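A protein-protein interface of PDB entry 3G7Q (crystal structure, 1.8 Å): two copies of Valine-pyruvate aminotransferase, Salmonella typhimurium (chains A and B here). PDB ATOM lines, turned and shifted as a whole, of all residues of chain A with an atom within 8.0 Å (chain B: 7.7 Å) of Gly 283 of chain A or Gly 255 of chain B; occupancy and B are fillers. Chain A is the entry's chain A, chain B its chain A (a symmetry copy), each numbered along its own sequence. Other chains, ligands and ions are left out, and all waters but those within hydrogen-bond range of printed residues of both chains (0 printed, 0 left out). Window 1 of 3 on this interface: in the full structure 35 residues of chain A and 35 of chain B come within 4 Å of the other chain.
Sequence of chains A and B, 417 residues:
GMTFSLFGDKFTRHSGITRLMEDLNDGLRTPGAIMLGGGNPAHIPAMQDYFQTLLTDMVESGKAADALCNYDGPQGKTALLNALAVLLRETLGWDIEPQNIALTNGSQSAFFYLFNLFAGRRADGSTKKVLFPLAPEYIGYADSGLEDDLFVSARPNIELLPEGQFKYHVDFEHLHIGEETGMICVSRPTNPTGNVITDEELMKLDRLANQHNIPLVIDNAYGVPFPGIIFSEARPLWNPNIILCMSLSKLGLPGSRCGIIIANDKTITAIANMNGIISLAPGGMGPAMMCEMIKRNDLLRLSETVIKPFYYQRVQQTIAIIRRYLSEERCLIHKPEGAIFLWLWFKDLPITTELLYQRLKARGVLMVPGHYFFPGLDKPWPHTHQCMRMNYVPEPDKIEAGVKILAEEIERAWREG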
ATOM      1  N   ALA A  64      -6.917 -13.371  -0.791  1.00  0.00           N
ATOM      2  CA  ALA A  64      -6.013 -13.588   0.325  1.00  0.00           C
ATOM      3  C   ALA A  64      -6.159 -12.439   1.314  1.00  0.00           C
ATOM      4  O   ALA A  64      -6.280 -12.655   2.526  1.00  0.00           O
ATOM      5  CB  ALA A  64      -4.569 -13.710  -0.142  1.00  0.00           C
ATOM      6  N   ALA A  65      -6.158 -11.218   0.791  1.00  0.00           N
ATOM      7  CA  ALA A  65      -6.330 -10.042   1.630  1.00  0.00           C
ATOM      8  C   ALA A  65      -7.689 -10.086   2.326  1.00  0.00           C
ATOM      9  O   ALA A  65      -7.779  -9.757   3.509  1.00  0.00           O
ATOM     10  CB  ALA A  65      -6.170  -8.746   0.819  1.00  0.00           C
ATOM     11  N   ASP A  66      -8.739 -10.499   1.617  1.00  0.00           N
ATOM     12  CA  ASP A  66     -10.077 -10.583   2.224  1.00  0.00           C
ATOM     13  C   ASP A  66     -10.077 -11.554   3.419  1.00  0.00           C
ATOM     14  O   ASP A  66     -10.698 -11.296   4.449  1.00  0.00           O
ATOM     15  CB  ASP A  66     -11.119 -11.072   1.229  1.00  0.00           C
ATOM     16  CG  ASP A  66     -11.516 -10.043   0.194  1.00  0.00           C
ATOM     17  OD1 ASP A  66     -11.199  -8.844   0.334  1.00  0.00           O
ATOM     18  OD2 ASP A  66     -12.190 -10.460  -0.782  1.00  0.00           O
ATOM     19  N   ALA A  67      -9.371 -12.649   3.257  1.00  0.00           N
ATOM     20  CA  ALA A  67      -9.277 -13.695   4.275  1.00  0.00           C
ATOM     21  C   ALA A  67      -8.578 -13.200   5.554  1.00  0.00           C
ATOM     22  O   ALA A  67      -8.963 -13.555   6.664  1.00  0.00           O
ATOM     23  CB  ALA A  67      -8.527 -14.882   3.702  1.00  0.00           C
ATOM     24  N   LEU A  68      -7.553 -12.373   5.395  1.00  0.00           N
ATOM     25  CA  LEU A  68      -6.784 -11.901   6.540  1.00  0.00           C
ATOM     26  C   LEU A  68      -7.314 -10.621   7.142  1.00  0.00           C
ATOM     27  O   LEU A  68      -7.210 -10.411   8.356  1.00  0.00           O
ATOM     28  CB  LEU A  68      -5.314 -11.727   6.118  1.00  0.00           C
ATOM     29  CG  LEU A  68      -4.592 -13.018   5.729  1.00  0.00           C
ATOM     30  CD1 LEU A  68      -3.367 -12.750   4.869  1.00  0.00           C
ATOM     31  CD2 LEU A  68      -4.220 -13.814   6.969  1.00  0.00           C
ATOM     32  N   CYS A  69      -7.878  -9.748   6.306  1.00  0.00           N
ATOM     33  CA  CYS A  69      -8.332  -8.444   6.747  1.00  0.00           C
ATOM     34  C   CYS A  69      -9.777  -8.358   7.229  1.00  0.00           C
ATOM     35  O   CYS A  69     -10.194  -7.295   7.670  1.00  0.00           O
ATOM     36  CB  CYS A  69      -8.093  -7.414   5.644  1.00  0.00           C
ATOM     37  SG  CYS A  69      -6.303  -7.306   5.238  1.00  0.00           S
ATOM     38  N   ASN A  70     -10.506  -9.469   7.141  1.00  0.00           N
ATOM     39  CA  ASN A  70     -11.896  -9.560   7.618  1.00  0.00           C
ATOM     40  C   ASN A  70     -12.047 -10.664   8.648  1.00  0.00           C
ATOM     41  O   ASN A  70     -11.490 -11.748   8.476  1.00  0.00           O
ATOM     42  CB  ASN A  70     -12.814  -9.803   6.453  1.00  0.00           C
ATOM     43  CG  ASN A  70     -12.880  -8.614   5.542  1.00  0.00           C
ATOM     44  OD1 ASN A  70     -12.432  -8.655   4.399  1.00  0.00           O
ATOM     45  ND2 ASN A  70     -13.422  -7.526   6.057  1.00  0.00           N
ATOM     46  N   TYR A  71     -12.785 -10.388   9.727  1.00  0.00           N
ATOM     47  CA  TYR A  71     -12.982 -11.389  10.793  1.00  0.00           C
ATOM     48  C   TYR A  71     -13.715 -12.604  10.233  1.00  0.00           C
ATOM     49  O   TYR A  71     -13.372 -13.746  10.563  1.00  0.00           O
ATOM     50  CB  TYR A  71     -13.748 -10.815  11.994  1.00  0.00           C
ATOM     51  CG  TYR A  71     -13.913 -11.807  13.138  1.00  0.00           C
ATOM     52  N   ASP A  72     -14.712 -12.345   9.387  1.00  0.00           N
ATOM     53  CA  ASP A  72     -15.464 -13.410   8.718  1.00  0.00           C
ATOM     54  C   ASP A  72     -15.773 -12.937   7.286  1.00  0.00           C
ATOM     55  O   ASP A  72     -16.882 -12.495   6.978  1.00  0.00           O
ATOM     56  CB  ASP A  72     -16.724 -13.754   9.525  1.00  0.00           C
ATOM     57  CG  ASP A  72     -17.519 -14.918   8.929  1.00  0.00           C
ATOM     58  OD1 ASP A  72     -16.954 -15.706   8.133  1.00  0.00           O
ATOM     59  OD2 ASP A  72     -18.720 -15.031   9.267  1.00  0.00           O
ATOM     60  N   GLY A  73     -14.768 -13.041   6.418  1.00  0.00           N
ATOM     61  CA  GLY A  73     -14.864 -12.550   5.042  1.00  0.00           C
ATOM     62  C   GLY A  73     -15.757 -13.352   4.114  1.00  0.00           C
ATOM     63  O   GLY A  73     -16.424 -14.291   4.559  1.00  0.00           O
ATOM     64  N   GLN A  75     -15.063 -15.591   2.044  1.00  0.00           N
ATOM     65  CA  GLN A  75     -14.694 -17.005   2.057  1.00  0.00           C
ATOM     66  C   GLN A  75     -14.322 -17.394   3.484  1.00  0.00           C
ATOM     67  O   GLN A  75     -13.434 -18.235   3.708  1.00  0.00           O
ATOM     68  CB  GLN A  75     -13.541 -17.271   1.108  1.00  0.00           C
ATOM     69  CG  GLN A  75     -13.870 -17.005  -0.332  1.00  0.00           C
ATOM     70  CD  GLN A  75     -12.718 -17.379  -1.226  1.00  0.00           C
ATOM     71  OE1 GLN A  75     -11.592 -16.930  -1.005  1.00  0.00           O
ATOM     72  NE2 GLN A  75     -12.986 -18.200  -2.248  1.00  0.00           N
ATOM     73  N   GLY A  76     -15.034 -16.786   4.438  1.00  0.00           N
ATOM     74  CA  GLY A  76     -14.802 -17.002   5.853  1.00  0.00           C
ATOM     75  C   GLY A  76     -15.514 -18.234   6.350  1.00  0.00           C
ATOM     76  O   GLY A  76     -16.046 -19.020   5.543  1.00  0.00           O
ATOM     77  N   LYS A  77     -15.510 -18.396   7.676  1.00  0.00           N
ATOM     78  CA  LYS A  77     -16.178 -19.507   8.337  1.00  0.00           C
ATOM     79  C   LYS A  77     -17.550 -19.780   7.715  1.00  0.00           C
ATOM     80  O   LYS A  77     -17.831 -20.910   7.325  1.00  0.00           O
ATOM     81  CB  LYS A  77     -16.327 -19.249   9.842  1.00  0.00           C
ATOM     82  N   LEU A  80     -17.520 -21.220   4.148  1.00  0.00           N
ATOM     83  CA  LEU A  80     -16.970 -22.580   4.234  1.00  0.00           C
ATOM     84  C   LEU A  80     -17.977 -23.575   4.812  1.00  0.00           C
ATOM     85  O   LEU A  80     -18.053 -24.710   4.341  1.00  0.00           O
ATOM     86  CB  LEU A  80     -15.686 -22.603   5.058  1.00  0.00           C
ATOM     87  CG  LEU A  80     -15.029 -23.977   5.218  1.00  0.00           C
ATOM     88  CD1 LEU A  80     -14.692 -24.577   3.856  1.00  0.00           C
ATOM     89  CD2 LEU A  80     -13.797 -23.899   6.094  1.00  0.00           C
ATOM     90  N   LEU A 103     -16.171 -25.053  13.090  1.00  0.00           N
ATOM     91  CA  LEU A 103     -14.763 -24.984  12.752  1.00  0.00           C
ATOM     92  C   LEU A 103     -13.967 -24.684  14.009  1.00  0.00           C
ATOM     93  O   LEU A 103     -14.463 -24.001  14.902  1.00  0.00           O
ATOM     94  CB  LEU A 103     -14.518 -23.893  11.723  1.00  0.00           C
ATOM     95  CG  LEU A 103     -15.343 -23.948  10.443  1.00  0.00           C
ATOM     96  CD1 LEU A 103     -14.981 -22.777   9.541  1.00  0.00           C
ATOM     97  CD2 LEU A 103     -15.109 -25.284   9.738  1.00  0.00           C
ATOM     98  N   THR A 104     -12.740 -25.200  14.085  1.00  0.00           N
ATOM     99  CA  THR A 104     -11.866 -24.976  15.226  1.00  0.00           C
ATOM    100  C   THR A 104     -10.466 -24.714  14.678  1.00  0.00           C
ATOM    101  O   THR A 104     -10.257 -24.778  13.478  1.00  0.00           O
ATOM    102  CB  THR A 104     -11.781 -26.216  16.144  1.00  0.00           C
ATOM    103  OG1 THR A 104     -11.133 -27.272  15.423  1.00  0.00           O
ATOM    104  CG2 THR A 104     -13.186 -26.671  16.640  1.00  0.00           C
ATOM    105  N   ASN A 105      -9.537 -24.491  15.603  1.00  0.00           N
ATOM    106  CA  ASN A 105      -8.123 -24.246  15.335  1.00  0.00           C
ATOM    107  C   ASN A 105      -7.373 -25.500  14.915  1.00  0.00           C
ATOM    108  O   ASN A 105      -6.216 -25.431  14.501  1.00  0.00           O
ATOM    109  CB  ASN A 105      -7.476 -23.699  16.624  1.00  0.00           C
ATOM    110  CG  ASN A 105      -6.191 -22.947  16.370  1.00  0.00           C
ATOM    111  OD1 ASN A 105      -5.161 -23.224  16.985  1.00  0.00           O
ATOM    112  ND2 ASN A 105      -6.239 -22.000  15.452  1.00  0.00           N
ATOM    113  N   LEU A 248      -7.674 -29.750   7.810  1.00  0.00           N
ATOM    114  CA  LEU A 248      -6.980 -29.368   6.588  1.00  0.00           C
ATOM    115  C   LEU A 248      -5.478 -29.666   6.640  1.00  0.00           C
ATOM    116  O   LEU A 248      -4.840 -29.778   5.612  1.00  0.00           O
ATOM    117  CB  LEU A 248      -7.184 -27.869   6.408  1.00  0.00           C
ATOM    118  CG  LEU A 248      -6.831 -27.166   5.120  1.00  0.00           C
ATOM    119  CD1 LEU A 248      -7.455 -27.820   3.902  1.00  0.00           C
ATOM    120  CD2 LEU A 248      -7.316 -25.699   5.281  1.00  0.00           C
ATOM    121  N   SER A 256      -1.811 -23.933   8.337  1.00  0.00           N
ATOM    122  CA  SER A 256      -3.160 -23.373   8.424  1.00  0.00           C
ATOM    123  C   SER A 256      -3.723 -23.966   9.709  1.00  0.00           C
ATOM    124  O   SER A 256      -3.191 -24.922  10.256  1.00  0.00           O
ATOM    125  CB  SER A 256      -4.053 -23.801   7.286  1.00  0.00           C
ATOM    126  OG  SER A 256      -4.410 -25.167   7.475  1.00  0.00           O
ATOM    127  N   ARG A 257      -4.815 -23.443  10.201  1.00  0.00           N
ATOM    128  CA  ARG A 257      -5.328 -23.973  11.459  1.00  0.00           C
ATOM    129  C   ARG A 257      -6.778 -24.121  11.254  1.00  0.00           C
ATOM    130  O   ARG A 257      -7.542 -23.215  11.612  1.00  0.00           O
ATOM    131  CB  ARG A 257      -5.016 -22.995  12.600  1.00  0.00           C
ATOM    132  CG  ARG A 257      -3.582 -23.028  13.082  1.00  0.00           C
ATOM    133  CD  ARG A 257      -3.247 -24.351  13.752  1.00  0.00           C
ATOM    134  NE  ARG A 257      -1.945 -24.320  14.405  1.00  0.00           N
ATOM    135  CZ  ARG A 257      -0.774 -24.419  13.785  1.00  0.00           C
ATOM    136  NH1 ARG A 257      -0.707 -24.530  12.462  1.00  0.00           N
ATOM    137  NH2 ARG A 257       0.352 -24.380  14.495  1.00  0.00           N
ATOM    138  N   CYS A 258      -7.169 -25.239  10.643  1.00  0.00           N
ATOM    139  CA  CYS A 258      -8.562 -25.432  10.339  1.00  0.00           C
ATOM    140  C   CYS A 258      -9.106 -26.840  10.616  1.00  0.00           C
ATOM    141  O   CYS A 258      -8.990 -27.739   9.783  1.00  0.00           O
ATOM    142  CB  CYS A 258      -8.796 -25.043   8.897  1.00  0.00           C
ATOM    143  SG  CYS A 258     -10.503 -24.820   8.592  1.00  0.00           S
ATOM    144  N   GLY A 259      -9.672 -26.995  11.807  1.00  0.00           N
ATOM    145  CA  GLY A 259     -10.336 -28.213  12.247  1.00  0.00           C
ATOM    146  C   GLY A 259     -11.825 -28.102  11.940  1.00  0.00           C
ATOM    147  O   GLY A 259     -12.402 -27.006  11.953  1.00  0.00           O
ATOM    148  N   LEU A 280     -10.832 -20.565  20.068  1.00  0.00           N
ATOM    149  CA  LEU A 280      -9.909 -21.335  19.289  1.00  0.00           C
ATOM    150  C   LEU A 280     -10.564 -21.593  17.914  1.00  0.00           C
ATOM    151  O   LEU A 280     -10.665 -22.747  17.468  1.00  0.00           O
ATOM    152  CB  LEU A 280      -9.546 -22.627  20.025  1.00  0.00           C
ATOM    153  N   ALA A 281     -11.022 -20.500  17.276  1.00  0.00           N
ATOM    154  CA  ALA A 281     -11.622 -20.524  15.930  1.00  0.00           C
ATOM    155  C   ALA A 281     -10.480 -20.515  14.928  1.00  0.00           C
ATOM    156  O   ALA A 281      -9.351 -20.138  15.288  1.00  0.00           O
ATOM    157  CB  ALA A 281     -12.509 -19.315  15.718  1.00  0.00           C
ATOM    158  N   PRO A 282     -10.740 -20.919  13.670  1.00  0.00           N
ATOM    159  CA  PRO A 282      -9.619 -20.928  12.744  1.00  0.00           C
ATOM    160  C   PRO A 282      -9.306 -19.539  12.184  1.00  0.00           C
ATOM    161  O   PRO A 282     -10.181 -18.698  12.133  1.00  0.00           O
ATOM    162  CB  PRO A 282     -10.131 -21.822  11.614  1.00  0.00           C
ATOM    163  CG  PRO A 282     -11.550 -21.552  11.567  1.00  0.00           C
ATOM    164  CD  PRO A 282     -11.976 -21.371  13.014  1.00  0.00           C
ATOM    165  N   GLY A 283      -8.071 -19.324  11.741  1.00  0.00           N
ATOM    166  CA  GLY A 283      -7.729 -18.077  11.032  1.00  0.00           C
ATOM    167  C   GLY A 283      -8.429 -18.108   9.665  1.00  0.00           C
ATOM    168  O   GLY A 283      -9.075 -19.091   9.313  1.00  0.00           O
ATOM    169  N   GLY A 284      -8.292 -17.049   8.887  1.00  0.00           N
ATOM    170  CA  GLY A 284      -8.983 -16.941   7.618  1.00  0.00           C
ATOM    171  C   GLY A 284      -8.401 -17.635   6.404  1.00  0.00           C
ATOM    172  O   GLY A 284      -9.152 -17.989   5.494  1.00  0.00           O
ATOM    173  N   MET A 285      -7.100 -17.875   6.384  1.00  0.00           N
ATOM    174  CA  MET A 285      -6.462 -18.381   5.181  1.00  0.00           C
ATOM    175  C   MET A 285      -6.870 -19.844   4.851  1.00  0.00           C
ATOM    176  O   MET A 285      -7.180 -20.157   3.701  1.00  0.00           O
ATOM    177  CB  MET A 285      -4.959 -18.216   5.309  1.00  0.00           C
ATOM    178  CG  MET A 285      -4.271 -18.062   4.006  1.00  0.00           C
ATOM    179  SD  MET A 285      -4.794 -16.421   3.048  1.00  0.00           S
ATOM    180  CE  MET A 285      -4.528 -17.246   1.570  1.00  0.00           C
ATOM    181  N   GLY A 286      -6.909 -20.696   5.875  1.00  0.00           N
ATOM    182  CA  GLY A 286      -7.335 -22.105   5.719  1.00  0.00           C
ATOM    183  C   GLY A 286      -8.727 -22.218   5.129  1.00  0.00           C
ATOM    184  O   GLY A 286      -8.890 -22.822   4.063  1.00  0.00           O
ATOM    185  N   PRO A 287      -9.739 -21.671   5.823  1.00  0.00           N
ATOM    186  CA  PRO A 287     -11.079 -21.686   5.260  1.00  0.00           C
ATOM    187  C   PRO A 287     -11.179 -21.121   3.843  1.00  0.00           C
ATOM    188  O   PRO A 287     -11.908 -21.696   3.020  1.00  0.00           O
ATOM    189  CB  PRO A 287     -11.890 -20.839   6.242  1.00  0.00           C
ATOM    190  CG  PRO A 287     -11.143 -20.937   7.530  1.00  0.00           C
ATOM    191  CD  PRO A 287      -9.709 -21.085   7.174  1.00  0.00           C
ATOM    192  N   ALA A 288     -10.451 -20.038   3.542  1.00  0.00           N
ATOM    193  CA  ALA A 288     -10.519 -19.433   2.213  1.00  0.00           C
ATOM    194  C   ALA A 288      -9.937 -20.377   1.166  1.00  0.00           C
ATOM    195  O   ALA A 288     -10.513 -20.556   0.078  1.00  0.00           O
ATOM    196  CB  ALA A 288      -9.808 -18.049   2.182  1.00  0.00           C
ATOM    197  N   ASN B  40     -14.658  -5.240  15.788  1.00  0.00           N
ATOM    198  CA  ASN B  40     -13.699  -5.283  14.692  1.00  0.00           C
ATOM    199  C   ASN B  40     -13.079  -3.943  14.346  1.00  0.00           C
ATOM    200  O   ASN B  40     -13.729  -2.900  14.407  1.00  0.00           O
ATOM    201  CB  ASN B  40     -14.349  -5.879  13.476  1.00  0.00           C
ATOM    202  CG  ASN B  40     -14.688  -7.352  13.685  1.00  0.00           C
ATOM    203  OD1 ASN B  40     -13.956  -8.097  14.372  1.00  0.00           O
ATOM    204  ND2 ASN B  40     -15.775  -7.772  13.093  1.00  0.00           N
ATOM    205  N   PRO B  41     -11.812  -3.970  13.928  1.00  0.00           N
ATOM    206  CA  PRO B  41     -11.165  -2.739  13.550  1.00  0.00           C
ATOM    207  C   PRO B  41     -11.661  -2.221  12.202  1.00  0.00           C
ATOM    208  O   PRO B  41     -12.452  -2.878  11.491  1.00  0.00           O
ATOM    209  CB  PRO B  41      -9.674  -3.134  13.474  1.00  0.00           C
ATOM    210  CG  PRO B  41      -9.683  -4.574  13.172  1.00  0.00           C
ATOM    211  CD  PRO B  41     -10.919  -5.140  13.821  1.00  0.00           C
ATOM    212  N   ASN B 105      -3.437 -18.259  19.737  1.00  0.00           N
ATOM    213  CA  ASN B 105      -4.445 -18.040  18.705  1.00  0.00           C
ATOM    214  C   ASN B 105      -5.090 -16.666  18.790  1.00  0.00           C
ATOM    215  O   ASN B 105      -5.840 -16.267  17.899  1.00  0.00           O
ATOM    216  CB  ASN B 105      -5.545 -19.107  18.871  1.00  0.00           C
ATOM    217  CG  ASN B 105      -6.360 -19.319  17.616  1.00  0.00           C
ATOM    218  OD1 ASN B 105      -7.590 -19.271  17.642  1.00  0.00           O
ATOM    219  ND2 ASN B 105      -5.679 -19.540  16.508  1.00  0.00           N
ATOM    220  N   LEU B 248      -1.994  -9.208  16.936  1.00  0.00           N
ATOM    221  CA  LEU B 248      -1.885  -8.670  15.587  1.00  0.00           C
ATOM    222  C   LEU B 248      -3.229  -8.190  15.029  1.00  0.00           C
ATOM    223  O   LEU B 248      -3.263  -7.385  14.121  1.00  0.00           O
ATOM    224  CB  LEU B 248      -1.350  -9.788  14.702  1.00  0.00           C
ATOM    225  CG  LEU B 248      -0.862  -9.526  13.297  1.00  0.00           C
ATOM    226  CD1 LEU B 248       0.164  -8.411  13.228  1.00  0.00           C
ATOM    227  CD2 LEU B 248      -0.268 -10.869  12.789  1.00  0.00           C
ATOM    228  N   SER B 249      -4.338  -8.634  15.596  1.00  0.00           N
ATOM    229  CA  SER B 249      -5.646  -8.387  14.975  1.00  0.00           C
ATOM    230  C   SER B 249      -6.036  -6.928  14.818  1.00  0.00           C
ATOM    231  O   SER B 249      -6.550  -6.532  13.762  1.00  0.00           O
ATOM    232  CB  SER B 249      -6.756  -9.129  15.729  1.00  0.00           C
ATOM    233  OG  SER B 249      -7.013  -8.527  16.962  1.00  0.00           O
ATOM    234  N   GLY B 252      -5.357  -4.563  11.864  1.00  0.00           N
ATOM    235  CA  GLY B 252      -6.194  -4.677  10.668  1.00  0.00           C
ATOM    236  C   GLY B 252      -6.104  -6.070  10.049  1.00  0.00           C
ATOM    237  O   GLY B 252      -6.370  -6.238   8.856  1.00  0.00           O
ATOM    238  N   LEU B 253      -5.745  -7.060  10.860  1.00  0.00           N
ATOM    239  CA  LEU B 253      -5.615  -8.443  10.426  1.00  0.00           C
ATOM    240  C   LEU B 253      -6.475  -9.348  11.310  1.00  0.00           C
ATOM    241  O   LEU B 253      -5.979 -10.329  11.860  1.00  0.00           O
ATOM    242  CB  LEU B 253      -4.147  -8.871  10.467  1.00  0.00           C
ATOM    243  CG  LEU B 253      -3.201  -8.116   9.524  1.00  0.00           C
ATOM    244  CD1 LEU B 253      -1.731  -8.448   9.792  1.00  0.00           C
ATOM    245  CD2 LEU B 253      -3.576  -8.401   8.026  1.00  0.00           C
ATOM    246  N   PRO B 254      -7.778  -9.033  11.417  1.00  0.00           N
ATOM    247  CA  PRO B 254      -8.641  -9.809  12.310  1.00  0.00           C
ATOM    248  C   PRO B 254      -8.807 -11.257  11.871  1.00  0.00           C
ATOM    249  O   PRO B 254      -9.235 -12.080  12.676  1.00  0.00           O
ATOM    250  CB  PRO B 254      -9.965  -9.044  12.247  1.00  0.00           C
ATOM    251  CG  PRO B 254      -9.969  -8.427  10.895  1.00  0.00           C
ATOM    252  CD  PRO B 254      -8.550  -7.981  10.728  1.00  0.00           C
ATOM    253  N   GLY B 255      -8.452 -11.550  10.618  1.00  0.00           N
ATOM    254  CA  GLY B 255      -8.444 -12.906  10.082  1.00  0.00           C
ATOM    255  C   GLY B 255      -7.177 -13.690  10.364  1.00  0.00           C
ATOM    256  O   GLY B 255      -7.113 -14.881  10.064  1.00  0.00           O
ATOM    257  N   SER B 256      -6.133 -13.048  10.885  1.00  0.00           N
ATOM    258  CA  SER B 256      -4.940 -13.787  11.300  1.00  0.00           C
ATOM    259  C   SER B 256      -5.230 -14.172  12.745  1.00  0.00           C
ATOM    260  O   SER B 256      -6.130 -13.638  13.378  1.00  0.00           O
ATOM    261  CB  SER B 256      -3.688 -12.947  11.286  1.00  0.00           C
ATOM    262  OG  SER B 256      -3.733 -12.042  12.385  1.00  0.00           O
ATOM    263  N   ARG B 257      -4.466 -15.072  13.306  1.00  0.00           N
ATOM    264  CA  ARG B 257      -4.772 -15.480  14.672  1.00  0.00           C
ATOM    265  C   ARG B 257      -3.474 -15.509  15.368  1.00  0.00           C
ATOM    266  O   ARG B 257      -2.850 -16.573  15.454  1.00  0.00           O
ATOM    267  CB  ARG B 257      -5.437 -16.864  14.663  1.00  0.00           C
ATOM    268  CG  ARG B 257      -6.894 -16.858  14.257  1.00  0.00           C
ATOM    269  CD  ARG B 257      -7.759 -16.143  15.283  1.00  0.00           C
ATOM    270  NE  ARG B 257      -9.181 -16.311  15.015  1.00  0.00           N
ATOM    271  CZ  ARG B 257      -9.868 -15.657  14.085  1.00  0.00           C
ATOM    272  NH1 ARG B 257      -9.271 -14.784  13.279  1.00  0.00           N
ATOM    273  NH2 ARG B 257     -11.170 -15.897  13.937  1.00  0.00           N
ATOM    274  N   CYS B 258      -3.039 -14.339  15.834  1.00  0.00           N
ATOM    275  CA  CYS B 258      -1.747 -14.264  16.464  1.00  0.00           C
ATOM    276  C   CYS B 258      -1.688 -13.410  17.738  1.00  0.00           C
ATOM    277  O   CYS B 258      -1.525 -12.191  17.678  1.00  0.00           O
ATOM    278  CB  CYS B 258      -0.746 -13.771  15.445  1.00  0.00           C
ATOM    279  SG  CYS B 258       0.886 -14.080  15.991  1.00  0.00           S
ATOM    280  N   PRO B 282      -0.789 -20.174  17.041  1.00  0.00           N
ATOM    281  CA  PRO B 282      -1.262 -19.423  15.890  1.00  0.00           C
ATOM    282  C   PRO B 282      -0.987 -20.136  14.566  1.00  0.00           C
ATOM    283  O   PRO B 282      -0.072 -20.932  14.488  1.00  0.00           O
ATOM    284  CB  PRO B 282      -0.419 -18.148  15.959  1.00  0.00           C
ATOM    285  CG  PRO B 282       0.848 -18.593  16.495  1.00  0.00           C
ATOM    286  CD  PRO B 282       0.502 -19.660  17.520  1.00  0.00           C
ATOM    287  N   GLY B 283      -1.762 -19.822  13.532  1.00  0.00           N
ATOM    288  CA  GLY B 283      -1.460 -20.332  12.181  1.00  0.00           C
ATOM    289  C   GLY B 283      -0.181 -19.636  11.692  1.00  0.00           C
ATOM    290  O   GLY B 283       0.362 -18.772  12.373  1.00  0.00           O
ATOM    291  N   MET B 285       0.415 -17.663   8.805  1.00  0.00           N
ATOM    292  CA  MET B 285       0.399 -16.443   8.016  1.00  0.00           C
ATOM    293  C   MET B 285       0.643 -15.168   8.869  1.00  0.00           C
ATOM    294  O   MET B 285       1.432 -14.304   8.484  1.00  0.00           O
ATOM    295  CB  MET B 285      -0.901 -16.374   7.235  1.00  0.00           C
ATOM    296  CG  MET B 285      -0.787 -15.609   5.971  1.00  0.00           C
ATOM    297  SD  MET B 285       0.439 -16.442   4.673  1.00  0.00           S
ATOM    298  CE  MET B 285       0.818 -14.878   4.086  1.00  0.00           C
ATOM    299  N   GLY B 286      -0.001 -15.098  10.034  1.00  0.00           N
ATOM    300  CA  GLY B 286       0.179 -13.972  10.975  1.00  0.00           C
ATOM    301  C   GLY B 286       1.630 -13.790  11.379  1.00  0.00           C
ATOM    302  O   GLY B 286       2.201 -12.720  11.140  1.00  0.00           O
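Gly 283 of chain A touches just these residues of chain B: Gly 255 and Arg 257.
Pro 254 of chain B touches just these residues of chain A: Leu 68, Cys 69, Asn 70 and Tyr 71.
Printed residues of chain B within 4 Å of Gly 284 of chain A: Gly 255 (2.7 Å).
Printed residues of chain A within 4 Å of Ser 256 of chain B: Leu 68 (3.8 Å).
Printed residues of chain B within 4 Å of Arg 257 of chain A: Pro 282 (3.5 Å) and Gly 283 (3.5 Å).
The nearest residue of chain B that does not touch Gly 283 of chain A is Ser 256 of chain B (4.9 Å).
The nearest residue of chain A that does not touch Gly 255 of chain B is Tyr 71 of chain A (4.5 Å).
The nearest printed residue of chain B that does not touch Asn 105 of chain A is Arg 257 of chain B (5.3 Å).
The backbone NH (N) of Gly 255 of chain B lies within hydrogen-bond range of the backbone carbonyl oxygen (O) of Leu 68 of chain A (2.8 Å).
The side-chain sulfur of Cys 69 of chain A lies close to the backbone carbonyl oxygen of Gly 252 of chain B, 3.8 Å away.
The side-chain amide nitrogen (ND2) of Asn 105 of chain B lies close to the side-chain amide nitrogen (ND2) of Asn 105 of chain A (2.7 Å).
NH2 of Arg 257 of chain A is in hydrogen-bond range of O of Pro 282 of chain B (3.5 Å).
The side-chain amide oxygen (OD1) of Asn 105 of chain B lies close to the backbone carbonyl oxygen (O) of Ala 281 of chain A, 3.1 Å away.
The backbone carbonyl oxygen of Pro 282 of chain A lies within hydrogen-bond range of the guanidinium group of Arg 257 of chain B.
The backbone NH (N) of Gly 284 of chain A sits at hydrogen-bond distance from the backbone carbonyl oxygen (O) of Gly 255 of chain B (2.7 Å).
The backbone carbonyl oxygen of Leu 68 of chain A sits close to the backbone nitrogen of Pro 254 of chain B, 3.4 Å away.
O of Leu 68 of chain A touches C of Leu 253 of chain B (3.2 Å).
Asn 70 of chain A touches Pro 254 of chain B (C to CG, 3.8 Å).
Ala 281 of chain A touches Arg 257 of chain B (O to NE, 3.8 Å).
CA of Gly 283 of chain A touches O of Gly 255 of chain B, 3.4 Å away.
Of the 16 printed residues of chain B, 10 touch a printed residue of chain A.
Hydrophobic or aromatic side chains of chain A within 4 Å of the printed part of chain B: Tyr 71.
Among the printed residues, no Asp or Glu carboxylate lies within 4 Å of a Lys or Arg side-chain nitrogen of the other chain.
Asn 105 of chain B touches its own counterpart, Asn 105 of chain A.
Arg 257 of chain A touches Pro 282 of chain B, and with the chains exchanged Pro 282 of chain A touches Arg 257 of chain B.
The side-chain amide oxygen of Asn 70 of chain A sits close to the backbone carbonyl oxygen of Asp 66 of chain A (3.2 Å).
O of Leu 253 of chain B sits at hydrogen-bond distance from OG of Ser 256 of chain B (2.9 Å).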
